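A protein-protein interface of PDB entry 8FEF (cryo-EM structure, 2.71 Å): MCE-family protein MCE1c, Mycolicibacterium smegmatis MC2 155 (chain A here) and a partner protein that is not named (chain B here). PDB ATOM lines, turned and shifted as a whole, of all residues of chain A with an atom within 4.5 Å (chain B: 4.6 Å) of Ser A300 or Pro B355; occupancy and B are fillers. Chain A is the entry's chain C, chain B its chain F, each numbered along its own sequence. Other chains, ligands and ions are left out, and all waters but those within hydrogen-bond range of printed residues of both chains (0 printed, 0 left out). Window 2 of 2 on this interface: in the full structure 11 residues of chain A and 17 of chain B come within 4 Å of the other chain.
The side-chain amino group (NZ) of Lys A305 is in hydrogen-bond range of the backbone carbonyl oxygen (O) of Pro B318.
The side-chain hydroxyl (OG) of Ser A300 sits close to the side-chain amino group (NZ) of Lys A305.
Among the printed residues, merely in contact across the chains: Ser A300 with Pro B355, Ser A300 with Asn B356 and Ser A300 with Ala B357.
Ser A300 touches just these residues of chain B: Pro B355, Asn B356 and Ala B357. Pro B355 touches just one residue of chain A: Ser A300 (3.6 Å). Printed residues of chain B within 4 Å of Lys A305: Pro B318 (3.1 Å). Of the printed residues of chain A, Pro B318 touches Lys A305 (3.1 Å). Of the printed residues of chain A, Asn B356 touches Ser A300 (3.5 Å). Leu A298 touches none of the printed residues of chain B. The nearest residue of chain B that does not touch Ser A300 is Pro B318 (4.2 Å). The nearest printed residue of chain A that does not touch Pro B355 is Ala A299 (5.4 Å).
Of the 7 printed residues of chain A, 2 touch a printed residue of chain B. Printed residues of chain A that touch a printed residue of chain B: Ser A300 and Lys A305. Of the 7 printed residues of chain B, 4 touch a printed residue of chain A. Printed residues of chain B that touch a printed residue of chain A: Pro B318, Pro B355, Asn B356 and Ala B357. Hydrophobic or aromatic side chains of chain B that line the printed part of chain A: Pro B318 and Ala B357. Among the printed residues, no Asp or Glu carboxylate lies within 4 Å of a Lys or Arg side-chain nitrogen of the other chain.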
ATOM      1  N   GLU A 296       4.482 -34.934  -5.843  1.00  0.00           N
ATOM      2  CA  GLU A 296       4.064 -34.324  -4.593  1.00  0.00           C
ATOM      3  C   GLU A 296       4.944 -33.145  -4.213  1.00  0.00           C
ATOM      4  O   GLU A 296       4.464 -32.146  -3.691  1.00  0.00           O
ATOM      5  CB  GLU A 296       4.026 -35.356  -3.470  1.00  0.00           C
ATOM      6  CG  GLU A 296       2.727 -35.346  -2.686  1.00  0.00           C
ATOM      7  CD  GLU A 296       1.523 -35.094  -3.576  1.00  0.00           C
ATOM      8  OE1 GLU A 296       1.593 -35.411  -4.777  1.00  0.00           O
ATOM      9  OE2 GLU A 296       0.505 -34.568  -3.086  1.00  0.00           O
ATOM     10  N   ALA A 297       6.242 -33.271  -4.474  1.00  0.00           N
ATOM     11  CA  ALA A 297       7.213 -32.239  -4.139  1.00  0.00           C
ATOM     12  C   ALA A 297       6.913 -30.958  -4.872  1.00  0.00           C
ATOM     13  O   ALA A 297       7.015 -29.887  -4.307  1.00  0.00           O
ATOM     14  CB  ALA A 297       8.609 -32.713  -4.470  1.00  0.00           C
ATOM     15  N   LEU A 298       6.531 -31.061  -6.132  1.00  0.00           N
ATOM     16  CA  LEU A 298       6.198 -29.893  -6.930  1.00  0.00           C
ATOM     17  C   LEU A 298       4.969 -29.125  -6.450  1.00  0.00           C
ATOM     18  O   LEU A 298       4.861 -27.945  -6.688  1.00  0.00           O
ATOM     19  CB  LEU A 298       5.999 -30.273  -8.393  1.00  0.00           C
ATOM     20  CG  LEU A 298       7.002 -31.159  -9.116  1.00  0.00           C
ATOM     21  CD1 LEU A 298       6.796 -31.007 -10.612  1.00  0.00           C
ATOM     22  CD2 LEU A 298       8.408 -30.758  -8.734  1.00  0.00           C
ATOM     23  N   ALA A 299       4.027 -29.818  -5.826  1.00  0.00           N
ATOM     24  CA  ALA A 299       2.741 -29.273  -5.371  1.00  0.00           C
ATOM     25  C   ALA A 299       2.653 -28.153  -4.330  1.00  0.00           C
ATOM     26  O   ALA A 299       1.812 -27.277  -4.450  1.00  0.00           O
ATOM     27  CB  ALA A 299       1.837 -30.414  -4.951  1.00  0.00           C
ATOM     28  N   SER A 300       3.519 -28.146  -3.332  1.00  0.00           N
ATOM     29  CA  SER A 300       3.424 -27.160  -2.250  1.00  0.00           C
ATOM     30  C   SER A 300       3.490 -25.698  -2.646  1.00  0.00           C
ATOM     31  O   SER A 300       2.843 -24.896  -2.020  1.00  0.00           O
ATOM     32  CB  SER A 300       4.480 -27.425  -1.173  1.00  0.00           C
ATOM     33  OG  SER A 300       4.516 -28.789  -0.782  1.00  0.00           O
ATOM     34  N   GLY A 301       4.305 -25.340  -3.629  1.00  0.00           N
ATOM     35  CA  GLY A 301       4.461 -23.957  -4.075  1.00  0.00           C
ATOM     36  C   GLY A 301       4.977 -23.930  -5.503  1.00  0.00           C
ATOM     37  O   GLY A 301       5.059 -24.969  -6.131  1.00  0.00           O
ATOM     38  N   LYS A 305      10.392 -28.924  -3.257  1.00  0.00           N
ATOM     39  CA  LYS A 305      11.167 -29.085  -2.038  1.00  0.00           C
ATOM     40  C   LYS A 305      12.340 -30.030  -2.271  1.00  0.00           C
ATOM     41  O   LYS A 305      12.249 -30.990  -3.039  1.00  0.00           O
ATOM     42  CB  LYS A 305      10.288 -29.615  -0.911  1.00  0.00           C
ATOM     43  CG  LYS A 305       9.066 -28.770  -0.627  1.00  0.00           C
ATOM     44  CD  LYS A 305       8.325 -29.286   0.590  1.00  0.00           C
ATOM     45  CE  LYS A 305       6.995 -28.585   0.750  1.00  0.00           C
ATOM     46  NZ  LYS A 305       7.163 -27.113   0.673  1.00  0.00           N
ATOM     47  N   PRO B 318       6.470 -22.917   2.914  1.00  0.00           N
ATOM     48  CA  PRO B 318       5.630 -24.074   3.225  1.00  0.00           C
ATOM     49  C   PRO B 318       6.443 -25.169   3.889  1.00  0.00           C
ATOM     50  O   PRO B 318       7.483 -25.592   3.361  1.00  0.00           O
ATOM     51  CB  PRO B 318       5.102 -24.514   1.853  1.00  0.00           C
ATOM     52  CG  PRO B 318       6.067 -23.991   0.871  1.00  0.00           C
ATOM     53  CD  PRO B 318       7.044 -23.085   1.563  1.00  0.00           C
ATOM     54  N   ASP B 353      -6.389 -28.887   3.204  1.00  0.00           N
ATOM     55  CA  ASP B 353      -6.401 -27.619   3.919  1.00  0.00           C
ATOM     56  C   ASP B 353      -5.021 -26.992   3.833  1.00  0.00           C
ATOM     57  O   ASP B 353      -4.039 -27.660   3.499  1.00  0.00           O
ATOM     58  CB  ASP B 353      -6.818 -27.804   5.385  1.00  0.00           C
ATOM     59  CG  ASP B 353      -5.705 -28.382   6.246  1.00  0.00           C
ATOM     60  OD1 ASP B 353      -4.933 -29.234   5.754  1.00  0.00           O
ATOM     61  OD2 ASP B 353      -5.603 -27.982   7.425  1.00  0.00           O
ATOM     62  N   ALA B 354      -4.971 -25.685   4.136  1.00  0.00           N
ATOM     63  CA  ALA B 354      -3.770 -24.860   4.242  1.00  0.00           C
ATOM     64  C   ALA B 354      -3.098 -24.698   2.882  1.00  0.00           C
ATOM     65  O   ALA B 354      -3.339 -25.496   1.969  1.00  0.00           O
ATOM     66  CB  ALA B 354      -2.794 -25.450   5.266  1.00  0.00           C
ATOM     67  N   PRO B 355      -2.276 -23.664   2.691  1.00  0.00           N
ATOM     68  CA  PRO B 355      -1.539 -23.552   1.422  1.00  0.00           C
ATOM     69  C   PRO B 355      -0.566 -24.693   1.173  1.00  0.00           C
ATOM     70  O   PRO B 355      -0.168 -24.903   0.021  1.00  0.00           O
ATOM     71  CB  PRO B 355      -0.806 -22.210   1.558  1.00  0.00           C
ATOM     72  CG  PRO B 355      -1.620 -21.437   2.534  1.00  0.00           C
ATOM     73  CD  PRO B 355      -2.153 -22.445   3.508  1.00  0.00           C
ATOM     74  N   ASN B 356      -0.171 -25.429   2.210  1.00  0.00           N
ATOM     75  CA  ASN B 356       0.834 -26.474   2.063  1.00  0.00           C
ATOM     76  C   ASN B 356       0.298 -27.624   1.221  1.00  0.00           C
ATOM     77  O   ASN B 356      -0.772 -28.165   1.510  1.00  0.00           O
ATOM     78  CB  ASN B 356       1.266 -26.981   3.435  1.00  0.00           C
ATOM     79  CG  ASN B 356       2.460 -27.905   3.364  1.00  0.00           C
ATOM     80  OD1 ASN B 356       3.154 -27.964   2.352  1.00  0.00           O
ATOM     81  ND2 ASN B 356       2.710 -28.630   4.447  1.00  0.00           N
ATOM     82  N   ALA B 357       1.050 -27.990   0.179  1.00  0.00           N
ATOM     83  CA  ALA B 357       0.731 -29.111  -0.709  1.00  0.00           C
ATOM     84  C   ALA B 357      -0.701 -29.038  -1.234  1.00  0.00           C
ATOM     85  O   ALA B 357      -1.450 -30.016  -1.207  1.00  0.00           O
ATOM     86  CB  ALA B 357       0.988 -30.446  -0.014  1.00  0.00           C
ATOM     87  N   VAL B 358      -1.087 -27.848  -1.699  1.00  0.00           N
ATOM     88  CA  VAL B 358      -2.438 -27.657  -2.222  1.00  0.00           C
ATOM     89  C   VAL B 358      -2.653 -28.513  -3.462  1.00  0.00           C
ATOM     90  O   VAL B 358      -3.673 -29.198  -3.597  1.00  0.00           O
ATOM     91  CB  VAL B 358      -2.696 -26.167  -2.508  1.00  0.00           C
ATOM     92  CG1 VAL B 358      -3.718 -25.995  -3.619  1.00  0.00           C
ATOM     93  CG2 VAL B 358      -3.169 -25.481  -1.254  1.00  0.00           C
